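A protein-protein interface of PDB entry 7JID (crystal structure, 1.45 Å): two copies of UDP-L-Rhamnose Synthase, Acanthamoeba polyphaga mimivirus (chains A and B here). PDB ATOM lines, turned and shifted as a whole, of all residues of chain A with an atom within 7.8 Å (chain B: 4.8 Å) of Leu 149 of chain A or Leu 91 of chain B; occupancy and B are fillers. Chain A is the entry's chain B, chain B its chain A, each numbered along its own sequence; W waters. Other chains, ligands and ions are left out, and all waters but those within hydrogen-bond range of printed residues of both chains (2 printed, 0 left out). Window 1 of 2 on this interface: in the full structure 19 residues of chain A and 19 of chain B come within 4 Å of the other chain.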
ATOM      1  N   LEU A  87      12.498 -15.038  31.408  1.00  0.00           N
ATOM      2  CA  LEU A  87      11.245 -14.412  30.957  1.00  0.00           C
ATOM      3  C   LEU A  87      10.071 -15.404  30.973  1.00  0.00           C
ATOM      4  O   LEU A  87       9.019 -15.104  31.589  1.00  0.00           O
ATOM      5  CB  LEU A  87      11.475 -13.772  29.579  1.00  0.00           C
ATOM      6  CG  LEU A  87      10.313 -12.940  29.050  1.00  0.00           C
ATOM      7  CD1 LEU A  87      10.918 -11.921  28.092  1.00  0.00           C
ATOM      8  CD2 LEU A  87       9.261 -13.799  28.341  1.00  0.00           C
ATOM      9  N   TYR A  88      10.155 -16.491  30.217  1.00  0.00           N
ATOM     10  CA  TYR A  88       8.954 -17.323  30.008  1.00  0.00           C
ATOM     11  C   TYR A  88       8.509 -17.981  31.320  1.00  0.00           C
ATOM     12  O   TYR A  88       7.341 -17.890  31.664  1.00  0.00           O
ATOM     13  CB  TYR A  88       9.195 -18.392  28.943  1.00  0.00           C
ATOM     14  CG  TYR A  88       7.958 -19.219  28.703  1.00  0.00           C
ATOM     15  CD1 TYR A  88       6.892 -18.698  28.008  1.00  0.00           C
ATOM     16  CD2 TYR A  88       7.848 -20.506  29.180  1.00  0.00           C
ATOM     17  CE1 TYR A  88       5.757 -19.446  27.754  1.00  0.00           C
ATOM     18  CE2 TYR A  88       6.708 -21.267  28.967  1.00  0.00           C
ATOM     19  CZ  TYR A  88       5.642 -20.721  28.275  1.00  0.00           C
ATOM     20  OH  TYR A  88       4.473 -21.406  28.068  1.00  0.00           O
ATOM     21  N   LEU A  91       6.704 -15.525  33.490  1.00  0.00           N
ATOM     22  CA  LEU A  91       5.394 -15.149  32.925  1.00  0.00           C
ATOM     23  C   LEU A  91       4.405 -16.295  33.190  1.00  0.00           C
ATOM     24  O   LEU A  91       3.278 -15.993  33.496  1.00  0.00           O
ATOM     25  CB  LEU A  91       5.503 -14.823  31.441  1.00  0.00           C
ATOM     26  CG  LEU A  91       5.584 -13.333  31.124  1.00  0.00           C
ATOM     27  CD1 LEU A  91       4.260 -12.637  31.423  1.00  0.00           C
ATOM     28  CD2 LEU A  91       6.674 -12.662  31.903  1.00  0.00           C
ATOM     29  N   ALA A  94       3.221 -15.774  36.656  1.00  0.00           N
ATOM     30  CA  ALA A  94       2.293 -14.624  36.706  1.00  0.00           C
ATOM     31  C   ALA A  94       0.917 -15.061  36.193  1.00  0.00           C
ATOM     32  O   ALA A  94      -0.082 -14.835  36.904  1.00  0.00           O
ATOM     33  CB  ALA A  94       2.846 -13.460  35.905  1.00  0.00           C
ATOM     34  N   PHE A  95       0.817 -15.675  35.014  1.00  0.00           N
ATOM     35  CA  PHE A  95      -0.505 -16.043  34.424  1.00  0.00           C
ATOM     36  C   PHE A  95      -1.275 -16.995  35.343  1.00  0.00           C
ATOM     37  O   PHE A  95      -2.491 -16.825  35.528  1.00  0.00           O
ATOM     38  CB  PHE A  95      -0.362 -16.703  33.046  1.00  0.00           C
ATOM     39  CG  PHE A  95      -0.165 -15.724  31.922  1.00  0.00           C
ATOM     40  CD1 PHE A  95      -1.164 -14.864  31.529  1.00  0.00           C
ATOM     41  CD2 PHE A  95       1.022 -15.690  31.216  1.00  0.00           C
ATOM     42  CE1 PHE A  95      -0.971 -13.934  30.518  1.00  0.00           C
ATOM     43  CE2 PHE A  95       1.211 -14.785  30.199  1.00  0.00           C
ATOM     44  CZ  PHE A  95       0.219 -13.924  29.825  1.00  0.00           C
ATOM     45  N   VAL A 142      16.770  -9.239  28.164  1.00  0.00           N
ATOM     46  CA  VAL A 142      15.619 -10.135  28.443  1.00  0.00           C
ATOM     47  C   VAL A 142      14.905  -9.704  29.726  1.00  0.00           C
ATOM     48  O   VAL A 142      13.697  -9.599  29.719  1.00  0.00           O
ATOM     49  CB  VAL A 142      16.101 -11.589  28.479  1.00  0.00           C
ATOM     50  CG1 VAL A 142      15.038 -12.506  29.069  1.00  0.00           C
ATOM     51  CG2 VAL A 142      16.446 -12.014  27.072  1.00  0.00           C
ATOM     52  N   LYS A 143      15.661  -9.417  30.782  1.00  0.00           N
ATOM     53  CA  LYS A 143      15.097  -9.073  32.113  1.00  0.00           C
ATOM     54  C   LYS A 143      14.336  -7.768  32.033  1.00  0.00           C
ATOM     55  O   LYS A 143      13.368  -7.615  32.796  1.00  0.00           O
ATOM     56  CB  LYS A 143      16.176  -9.002  33.176  1.00  0.00           C
ATOM     57  CG  LYS A 143      16.503 -10.385  33.711  1.00  0.00           C
ATOM     58  CD  LYS A 143      15.404 -10.909  34.550  1.00  0.00           C
ATOM     59  CE  LYS A 143      15.863 -12.149  35.256  1.00  0.00           C
ATOM     60  NZ  LYS A 143      14.877 -12.615  36.253  1.00  0.00           N
ATOM     61  N   GLY A 144      14.779  -6.867  31.151  1.00  0.00           N
ATOM     62  CA  GLY A 144      14.052  -5.620  30.930  1.00  0.00           C
ATOM     63  C   GLY A 144      12.672  -5.902  30.400  1.00  0.00           C
ATOM     64  O   GLY A 144      11.670  -5.212  30.817  1.00  0.00           O
ATOM     65  N   PHE A 145      12.567  -6.786  29.409  1.00  0.00           N
ATOM     66  CA  PHE A 145      11.246  -7.160  28.874  1.00  0.00           C
ATOM     67  C   PHE A 145      10.436  -7.881  29.948  1.00  0.00           C
ATOM     68  O   PHE A 145       9.249  -7.626  30.029  1.00  0.00           O
ATOM     69  CB  PHE A 145      11.334  -7.937  27.578  1.00  0.00           C
ATOM     70  CG  PHE A 145      11.761  -7.036  26.455  1.00  0.00           C
ATOM     71  CD1 PHE A 145      10.866  -6.096  25.969  1.00  0.00           C
ATOM     72  CD2 PHE A 145      13.030  -7.089  25.919  1.00  0.00           C
ATOM     73  CE1 PHE A 145      11.221  -5.235  24.940  1.00  0.00           C
ATOM     74  CE2 PHE A 145      13.368  -6.241  24.877  1.00  0.00           C
ATOM     75  CZ  PHE A 145      12.476  -5.317  24.393  1.00  0.00           C
ATOM     76  N   THR A 146      11.028  -8.732  30.759  1.00  0.00           N
ATOM     77  CA  THR A 146      10.255  -9.409  31.829  1.00  0.00           C
ATOM     78  C   THR A 146       9.685  -8.328  32.760  1.00  0.00           C
ATOM     79  O   THR A 146       8.479  -8.371  33.143  1.00  0.00           O
ATOM     80  CB  THR A 146      11.140 -10.385  32.596  1.00  0.00           C
ATOM     81  OG1 THR A 146      11.681 -11.283  31.631  1.00  0.00           O
ATOM     82  CG2 THR A 146      10.357 -11.166  33.636  1.00  0.00           C
ATOM     83  N   ASP A 147      10.516  -7.349  33.113  1.00  0.00           N
ATOM     84  CA  ASP A 147      10.076  -6.249  33.989  1.00  0.00           C
ATOM     85  C   ASP A 147       8.869  -5.534  33.389  1.00  0.00           C
ATOM     86  O   ASP A 147       7.878  -5.263  34.126  1.00  0.00           O
ATOM     87  CB  ASP A 147      11.197  -5.256  34.220  1.00  0.00           C
ATOM     88  CG  ASP A 147      10.845  -4.204  35.251  1.00  0.00           C
ATOM     89  OD1 ASP A 147      11.057  -4.488  36.461  1.00  0.00           O
ATOM     90  OD2 ASP A 147      10.408  -3.095  34.844  1.00  0.00           O
ATOM     91  N   ARG A 148       8.927  -5.184  32.105  1.00  0.00           N
ATOM     92  CA  ARG A 148       7.803  -4.487  31.429  1.00  0.00           C
ATOM     93  C   ARG A 148       6.582  -5.404  31.489  1.00  0.00           C
ATOM     94  O   ARG A 148       5.482  -4.920  31.808  1.00  0.00           O
ATOM     95  CB  ARG A 148       8.211  -4.119  30.014  1.00  0.00           C
ATOM     96  CG  ARG A 148       9.396  -3.169  30.000  1.00  0.00           C
ATOM     97  CD  ARG A 148       9.711  -2.801  28.581  1.00  0.00           C
ATOM     98  NE  ARG A 148       8.678  -1.946  28.058  1.00  0.00           N
ATOM     99  CZ  ARG A 148       8.657  -1.428  26.824  1.00  0.00           C
ATOM    100  NH1 ARG A 148       9.652  -1.652  25.980  1.00  0.00           N
ATOM    101  NH2 ARG A 148       7.649  -0.654  26.457  1.00  0.00           N
ATOM    102  N   LEU A 149       6.759  -6.693  31.222  1.00  0.00           N
ATOM    103  CA  LEU A 149       5.609  -7.637  31.152  1.00  0.00           C
ATOM    104  C   LEU A 149       4.951  -7.752  32.529  1.00  0.00           C
ATOM    105  O   LEU A 149       3.715  -7.832  32.618  1.00  0.00           O
ATOM    106  CB  LEU A 149       6.080  -8.990  30.569  1.00  0.00           C
ATOM    107  CG  LEU A 149       6.351  -8.971  29.056  1.00  0.00           C
ATOM    108  CD1 LEU A 149       7.173 -10.190  28.626  1.00  0.00           C
ATOM    109  CD2 LEU A 149       5.074  -8.905  28.253  1.00  0.00           C
ATOM    110  N   MET A 150       5.737  -7.618  33.590  1.00  0.00           N
ATOM    111  CA  MET A 150       5.215  -7.773  34.975  1.00  0.00           C
ATOM    112  C   MET A 150       4.278  -6.599  35.279  1.00  0.00           C
ATOM    113  O   MET A 150       3.373  -6.776  36.147  1.00  0.00           O
ATOM    114  CB  MET A 150       6.324  -7.899  36.016  1.00  0.00           C
ATOM    115  CG  MET A 150       7.048  -9.210  35.965  1.00  0.00           C
ATOM    116  SD  MET A 150       5.941 -10.617  36.315  1.00  0.00           S
ATOM    117  CE  MET A 150       7.056 -11.996  36.089  1.00  0.00           C
ATOM    118  N   HIS A 151       4.410  -5.480  34.568  1.00  0.00           N
ATOM    119  CA  HIS A 151       3.538  -4.294  34.761  1.00  0.00           C
ATOM    120  C   HIS A 151       2.105  -4.614  34.281  1.00  0.00           C
ATOM    121  O   HIS A 151       1.153  -3.852  34.634  1.00  0.00           O
ATOM    122  CB  HIS A 151       4.130  -3.036  34.124  1.00  0.00           C
ATOM    123  CG  HIS A 151       5.264  -2.404  34.893  1.00  0.00           C
ATOM    124  ND1 HIS A 151       6.535  -3.005  34.970  1.00  0.00           N
ATOM    125  CD2 HIS A 151       5.372  -1.210  35.532  1.00  0.00           C
ATOM    126  CE1 HIS A 151       7.349  -2.227  35.660  1.00  0.00           C
ATOM    127  NE2 HIS A 151       6.666  -1.093  36.020  1.00  0.00           N
ATOM    128  N   PHE A 152       1.898  -5.645  33.452  1.00  0.00           N
ATOM    129  CA  PHE A 152       0.522  -6.043  33.051  1.00  0.00           C
ATOM    130  C   PHE A 152      -0.149  -6.853  34.158  1.00  0.00           C
ATOM    131  O   PHE A 152      -1.352  -7.184  33.994  1.00  0.00           O
ATOM    132  CB  PHE A 152       0.493  -6.835  31.733  1.00  0.00           C
ATOM    133  CG  PHE A 152       0.837  -6.036  30.515  1.00  0.00           C
ATOM    134  CD1 PHE A 152      -0.108  -5.233  29.899  1.00  0.00           C
ATOM    135  CD2 PHE A 152       2.095  -6.159  29.937  1.00  0.00           C
ATOM    136  CE1 PHE A 152       0.225  -4.469  28.799  1.00  0.00           C
ATOM    137  CE2 PHE A 152       2.419  -5.414  28.820  1.00  0.00           C
ATOM    138  CZ  PHE A 152       1.488  -4.572  28.256  1.00  0.00           C
ATOM    139  N   PHE A 153       0.568  -7.145  35.251  1.00  0.00           N
ATOM    140  CA  PHE A 153       0.055  -7.909  36.419  1.00  0.00           C
ATOM    141  C   PHE A 153       0.162  -7.027  37.675  1.00  0.00           C
ATOM    142  O   PHE A 153       0.420  -7.536  38.719  1.00  0.00           O
ATOM    143  CB  PHE A 153       0.839  -9.209  36.555  1.00  0.00           C
ATOM    144  CG  PHE A 153       0.712 -10.157  35.391  1.00  0.00           C
ATOM    145  CD1 PHE A 153      -0.227 -11.161  35.398  1.00  0.00           C
ATOM    146  CD2 PHE A 153       1.614 -10.109  34.342  1.00  0.00           C
ATOM    147  CE1 PHE A 153      -0.345 -12.014  34.317  1.00  0.00           C
ATOM    148  CE2 PHE A 153       1.505 -10.964  33.254  1.00  0.00           C
ATOM    149  CZ  PHE A 153       0.551 -11.942  33.259  1.00  0.00           C
ATOM    150  N   ASP A 154      -0.100  -5.736  37.544  1.00  0.00           N
ATOM    151  CA  ASP A 154       0.228  -4.766  38.620  1.00  0.00           C
ATOM    152  C   ASP A 154      -0.644  -5.007  39.848  1.00  0.00           C
ATOM    153  O   ASP A 154      -0.187  -4.638  40.928  1.00  0.00           O
ATOM    154  CB  ASP A 154       0.047  -3.349  38.132  1.00  0.00           C
ATOM    155  CG  ASP A 154       0.654  -2.314  39.050  1.00  0.00           C
ATOM    156  OD1 ASP A 154       1.886  -2.295  39.163  1.00  0.00           O
ATOM    157  OD2 ASP A 154      -0.116  -1.510  39.594  1.00  0.00           O
ATOM    158  N   VAL A 157       0.888  -9.353  40.999  1.00  0.00           N
ATOM    159  CA  VAL A 157       2.300  -9.779  41.172  1.00  0.00           C
ATOM    160  C   VAL A 157       3.082  -8.624  41.815  1.00  0.00           C
ATOM    161  O   VAL A 157       2.927  -7.452  41.375  1.00  0.00           O
ATOM    162  CB  VAL A 157       2.918 -10.170  39.831  1.00  0.00           C
ATOM    163  CG1 VAL A 157       4.394 -10.494  39.951  1.00  0.00           C
ATOM    164  CG2 VAL A 157       2.115 -11.325  39.236  1.00  0.00           C
ATOM    165  N   ASN A 159       6.663  -7.360  41.913  1.00  0.00           N
ATOM    166  CA  ASN A 159       7.872  -7.364  41.072  1.00  0.00           C
ATOM    167  C   ASN A 159       8.946  -6.528  41.778  1.00  0.00           C
ATOM    168  O   ASN A 159       8.874  -5.284  41.717  1.00  0.00           O
ATOM    169  CB  ASN A 159       7.523  -6.839  39.673  1.00  0.00           C
ATOM    170  CG  ASN A 159       8.740  -6.535  38.828  1.00  0.00           C
ATOM    171  OD1 ASN A 159       9.705  -7.283  38.846  1.00  0.00           O
ATOM    172  ND2 ASN A 159       8.678  -5.459  38.049  1.00  0.00           N
ATOM    173  N   THR A 213       5.282  -3.014  41.047  1.00  0.00           N
ATOM    174  CA  THR A 213       6.746  -3.002  40.930  1.00  0.00           C
ATOM    175  C   THR A 213       7.324  -2.125  42.032  1.00  0.00           C
ATOM    176  O   THR A 213       6.756  -1.061  42.313  1.00  0.00           O
ATOM    177  CB  THR A 213       7.171  -2.451  39.576  1.00  0.00           C
ATOM    178  OG1 THR A 213       6.644  -3.344  38.591  1.00  0.00           O
ATOM    179  CG2 THR A 213       8.670  -2.339  39.431  1.00  0.00           C
ATOM    180  N   LEU B  87       8.303 -10.600  20.239  1.00  0.00           N
ATOM    181  CA  LEU B  87       7.625 -11.117  21.450  1.00  0.00           C
ATOM    182  C   LEU B  87       6.904  -9.977  22.156  1.00  0.00           C
ATOM    183  O   LEU B  87       5.667 -10.087  22.387  1.00  0.00           O
ATOM    184  CB  LEU B  87       8.658 -11.800  22.346  1.00  0.00           C
ATOM    185  CG  LEU B  87       8.094 -12.559  23.542  1.00  0.00           C
ATOM    186  CD1 LEU B  87       9.043 -13.685  23.906  1.00  0.00           C
ATOM    187  CD2 LEU B  87       7.871 -11.626  24.723  1.00  0.00           C
ATOM    188  N   TYR B  88       7.637  -8.979  22.660  1.00  0.00           N
ATOM    189  CA  TYR B  88       7.010  -7.951  23.513  1.00  0.00           C
ATOM    190  C   TYR B  88       5.835  -7.255  22.822  1.00  0.00           C
ATOM    191  O   TYR B  88       4.728  -7.160  23.461  1.00  0.00           O
ATOM    192  CB  TYR B  88       8.037  -6.960  24.058  1.00  0.00           C
ATOM    193  CG  TYR B  88       7.443  -6.001  25.063  1.00  0.00           C
ATOM    194  CD1 TYR B  88       7.052  -6.445  26.322  1.00  0.00           C
ATOM    195  CD2 TYR B  88       7.142  -4.707  24.718  1.00  0.00           C
ATOM    196  CE1 TYR B  88       6.460  -5.594  27.239  1.00  0.00           C
ATOM    197  CE2 TYR B  88       6.550  -3.836  25.634  1.00  0.00           C
ATOM    198  CZ  TYR B  88       6.175  -4.292  26.889  1.00  0.00           C
ATOM    199  OH  TYR B  88       5.527  -3.460  27.757  1.00  0.00           O
ATOM    200  N   GLY B  89       6.013  -6.685  21.625  1.00  0.00           N
ATOM    201  CA  GLY B  89       4.940  -5.987  20.893  1.00  0.00           C
ATOM    202  C   GLY B  89       3.706  -6.880  20.770  1.00  0.00           C
ATOM    203  O   GLY B  89       2.595  -6.470  21.132  1.00  0.00           O
ATOM    204  N   PRO B  90       3.839  -8.114  20.240  1.00  0.00           N
ATOM    205  CA  PRO B  90       2.686  -9.013  20.143  1.00  0.00           C
ATOM    206  C   PRO B  90       2.000  -9.264  21.501  1.00  0.00           C
ATOM    207  O   PRO B  90       0.791  -9.319  21.525  1.00  0.00           O
ATOM    208  CB  PRO B  90       3.336 -10.296  19.563  1.00  0.00           C
ATOM    209  CG  PRO B  90       4.438  -9.746  18.677  1.00  0.00           C
ATOM    210  CD  PRO B  90       5.041  -8.636  19.532  1.00  0.00           C
ATOM    211  N   LEU B  91       2.745  -9.405  22.589  1.00  0.00           N
ATOM    212  CA  LEU B  91       2.149  -9.650  23.911  1.00  0.00           C
ATOM    213  C   LEU B  91       1.362  -8.394  24.334  1.00  0.00           C
ATOM    214  O   LEU B  91       0.288  -8.571  24.966  1.00  0.00           O
ATOM    215  CB  LEU B  91       3.216 -10.037  24.920  1.00  0.00           C
ATOM    216  CG  LEU B  91       3.353 -11.531  25.192  1.00  0.00           C
ATOM    217  CD1 LEU B  91       2.162 -12.060  25.974  1.00  0.00           C
ATOM    218  CD2 LEU B  91       3.530 -12.303  23.907  1.00  0.00           C
ATOM    219  N   CYS B  92       1.878  -7.193  24.068  1.00  0.00           N
ATOM    220  CA  CYS B  92       1.188  -5.915  24.406  1.00  0.00           C
ATOM    221  C   CYS B  92      -0.177  -5.892  23.704  1.00  0.00           C
ATOM    222  O   CYS B  92      -1.245  -5.626  24.366  1.00  0.00           O
ATOM    223  CB  CYS B  92       2.010  -4.717  23.970  1.00  0.00           C
ATOM    224  SG  CYS B  92       3.435  -4.425  25.050  1.00  0.00           S
ATOM    225  N   LEU B  93      -0.193  -6.246  22.419  1.00  0.00           N
ATOM    226  CA  LEU B  93      -1.451  -6.344  21.648  1.00  0.00           C
ATOM    227  C   LEU B  93      -2.379  -7.379  22.267  1.00  0.00           C
ATOM    228  O   LEU B  93      -3.606  -7.069  22.434  1.00  0.00           O
ATOM    229  CB  LEU B  93      -1.126  -6.661  20.195  1.00  0.00           C
ATOM    230  CG  LEU B  93      -0.288  -5.651  19.420  1.00  0.00           C
ATOM    231  CD1 LEU B  93      -0.190  -6.121  17.994  1.00  0.00           C
ATOM    232  CD2 LEU B  93      -0.910  -4.259  19.436  1.00  0.00           C
ATOM    233  N   ALA B  94      -1.881  -8.556  22.663  1.00  0.00           N
ATOM    234  CA  ALA B  94      -2.715  -9.590  23.317  1.00  0.00           C
ATOM    235  C   ALA B  94      -3.337  -9.019  24.601  1.00  0.00           C
ATOM    236  O   ALA B  94      -4.590  -9.102  24.773  1.00  0.00           O
ATOM    237  CB  ALA B  94      -1.959 -10.839  23.620  1.00  0.00           C
ATOM    238  N   PHE B  95      -2.529  -8.433  25.469  1.00  0.00           N
ATOM    239  CA  PHE B  95      -3.035  -7.979  26.785  1.00  0.00           C
ATOM    240  C   PHE B  95      -4.101  -6.914  26.558  1.00  0.00           C
ATOM    241  O   PHE B  95      -5.138  -6.937  27.237  1.00  0.00           O
ATOM    242  CB  PHE B  95      -1.943  -7.377  27.660  1.00  0.00           C
ATOM    243  CG  PHE B  95      -1.125  -8.408  28.398  1.00  0.00           C
ATOM    244  CD1 PHE B  95      -1.689  -9.205  29.355  1.00  0.00           C
ATOM    245  CD2 PHE B  95       0.214  -8.588  28.111  1.00  0.00           C
ATOM    246  CE1 PHE B  95      -0.970 -10.194  30.004  1.00  0.00           C
ATOM    247  CE2 PHE B  95       0.947  -9.538  28.790  1.00  0.00           C
ATOM    248  CZ  PHE B  95       0.369 -10.362  29.718  1.00  0.00           C
ATOM    249  N   THR B 146       7.030 -16.716  21.968  1.00  0.00           N
ATOM    250  CA  THR B 146       5.798 -15.948  21.661  1.00  0.00           C
ATOM    251  C   THR B 146       4.634 -16.911  21.403  1.00  0.00           C
ATOM    252  O   THR B 146       3.495 -16.683  21.896  1.00  0.00           O
ATOM    253  CB  THR B 146       5.994 -14.999  20.490  1.00  0.00           C
ATOM    254  OG1 THR B 146       7.167 -14.270  20.862  1.00  0.00           O
ATOM    255  CG2 THR B 146       4.791 -14.118  20.288  1.00  0.00           C
ATOM    256  N   LEU B 149       3.388 -18.261  24.645  1.00  0.00           N
ATOM    257  CA  LEU B 149       2.712 -17.213  25.443  1.00  0.00           C
ATOM    258  C   LEU B 149       1.325 -16.961  24.872  1.00  0.00           C
ATOM    259  O   LEU B 149       0.361 -16.702  25.649  1.00  0.00           O
ATOM    260  CB  LEU B 149       3.557 -15.935  25.481  1.00  0.00           C
ATOM    261  CG  LEU B 149       4.795 -16.052  26.362  1.00  0.00           C
ATOM    262  CD1 LEU B 149       5.799 -14.957  26.037  1.00  0.00           C
ATOM    263  CD2 LEU B 149       4.390 -16.000  27.823  1.00  0.00           C
ATOM    264  N   MET B 150       1.155 -17.136  23.568  1.00  0.00           N
ATOM    265  CA  MET B 150      -0.174 -16.885  22.936  1.00  0.00           C
ATOM    266  C   MET B 150      -1.203 -17.921  23.394  1.00  0.00           C
ATOM    267  O   MET B 150      -2.408 -17.600  23.361  1.00  0.00           O
ATOM    268  CB  MET B 150      -0.100 -16.839  21.414  1.00  0.00           C
ATOM    269  CG  MET B 150       0.607 -15.619  20.898  1.00  0.00           C
ATOM    270  SD  MET B 150      -0.259 -14.058  21.316  1.00  0.00           S
ATOM    271  CE  MET B 150       0.923 -12.874  20.658  1.00  0.00           C
ATOM    272  N   PHE B 153      -3.781 -16.930  25.838  1.00  0.00           N
ATOM    273  CA  PHE B 153      -4.844 -16.074  25.289  1.00  0.00           C
ATOM    274  C   PHE B 153      -5.731 -16.879  24.318  1.00  0.00           C
ATOM    275  O   PHE B 153      -6.233 -16.329  23.376  1.00  0.00           O
ATOM    276  CB  PHE B 153      -4.238 -14.863  24.576  1.00  0.00           C
ATOM    277  CG  PHE B 153      -3.433 -13.954  25.460  1.00  0.00           C
ATOM    278  CD1 PHE B 153      -4.009 -12.836  26.033  1.00  0.00           C
ATOM    279  CD2 PHE B 153      -2.094 -14.209  25.697  1.00  0.00           C
ATOM    280  CE1 PHE B 153      -3.264 -12.006  26.854  1.00  0.00           C
ATOM    281  CE2 PHE B 153      -1.341 -13.366  26.505  1.00  0.00           C
ATOM    282  CZ  PHE B 153      -1.929 -12.257  27.066  1.00  0.00           C
HETATM  283  O   HOH W   1       4.251  -2.826  30.355  1.00  0.00           O
HETATM  284  O   HOH W   2       6.574  -0.971  29.837  1.00  0.00           O
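Among the printed residues, merely in contact across the chains: Tyr 88 of chain A with Leu 149 of chain B (3.7 Å), Leu 91 of chain A with Leu 149 of chain B (3.96 Å), Phe 95 of chain A with Phe 95 of chain B (3.6 Å), Phe 95 of chain A with Phe 153 of chain B (3.7 Å), Phe 145 of chain A with Tyr 88 of chain B (3.5 Å), Arg 148 of chain A with Tyr 88 of chain B (3.4 Å), Leu 149 of chain A with Tyr 88 of chain B (3.7 Å), Leu 149 of chain A with Leu 91 of chain B (3.98 Å), Phe 152 of chain A with Tyr 88 of chain B (3.8 Å), Phe 152 of chain A with Cys 92 of chain B (3.8 Å), Phe 152 of chain A with Phe 95 of chain B (3.6 Å) and Phe 153 of chain A with Phe 95 of chain B (3.8 Å).
Of the printed residues of chain B, Leu 149 of chain A touches Tyr 88 (3.7 Å) and Leu 91 (3.98 Å).
Of the printed residues of chain A, Leu 91 of chain B touches Leu 149.
Of the printed residues of chain A, Leu 149 of chain B touches Tyr 88 (3.7 Å) and Leu 91 (3.96 Å).
Of the printed residues of chain B, Tyr 88 of chain A touches Leu 149 (3.7 Å).
Of the printed residues of chain B, Arg 148 of chain A touches Tyr 88.
Ala 94 of chain A touches none of the printed residues of chain B.
The nearest printed residue of chain B that does not touch Leu 149 of chain A is Phe 95 of chain B (4.2 Å).
The nearest printed residue of chain A that does not touch Cys 92 of chain B is Leu 149 of chain A (5.5 Å).
Printed residues of chain A that touch a printed residue of chain B: Tyr 88, Leu 91, Phe 95, Phe 145, Arg 148, Leu 149, Phe 152 and Phe 153.
Hydrophobic or aromatic side chains of chain A that line the printed part of chain B: Tyr 88, Leu 91, Phe 95, Phe 145, Leu 149, Phe 152 and Phe 153.
Among the printed residues, 12 pairs touch across the chains.
Among the printed residues, no Asp or Glu carboxylate lies within 4 Å of a Lys or Arg side-chain nitrogen of the other chain.
Water W1 bridges the backbone carbonyl oxygen of Arg 148 of chain A and the side-chain hydroxyl of Tyr 88 of chain B.
Water W2 lies within hydrogen-bond range of the guanidinium group (NE) of Arg 148 of chain A and the side-chain hydroxyl (OH) of Tyr 88 of chain B.
Tyr 88 of chain A touches Leu 149 of chain B, and with the chains exchanged Leu 149 of chain A touches Tyr 88 of chain B.
Leu 91 of chain A touches Leu 149 of chain B, and with the chains exchanged Leu 149 of chain A touches Leu 91 of chain B.
Phe 95 of chain A touches its own counterpart, Phe 95 of chain B.
Phe 95 of chain A touches Phe 153 of chain B, and with the chains exchanged Phe 153 of chain A touches Phe 95 of chain B.
Positions printed for both chains: 87, 88, 91, 94, 95, 146, 149, 150 and 153.
O of Tyr 88 of chain B sits close to SG of Cys 92 of chain B (3.4 Å).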
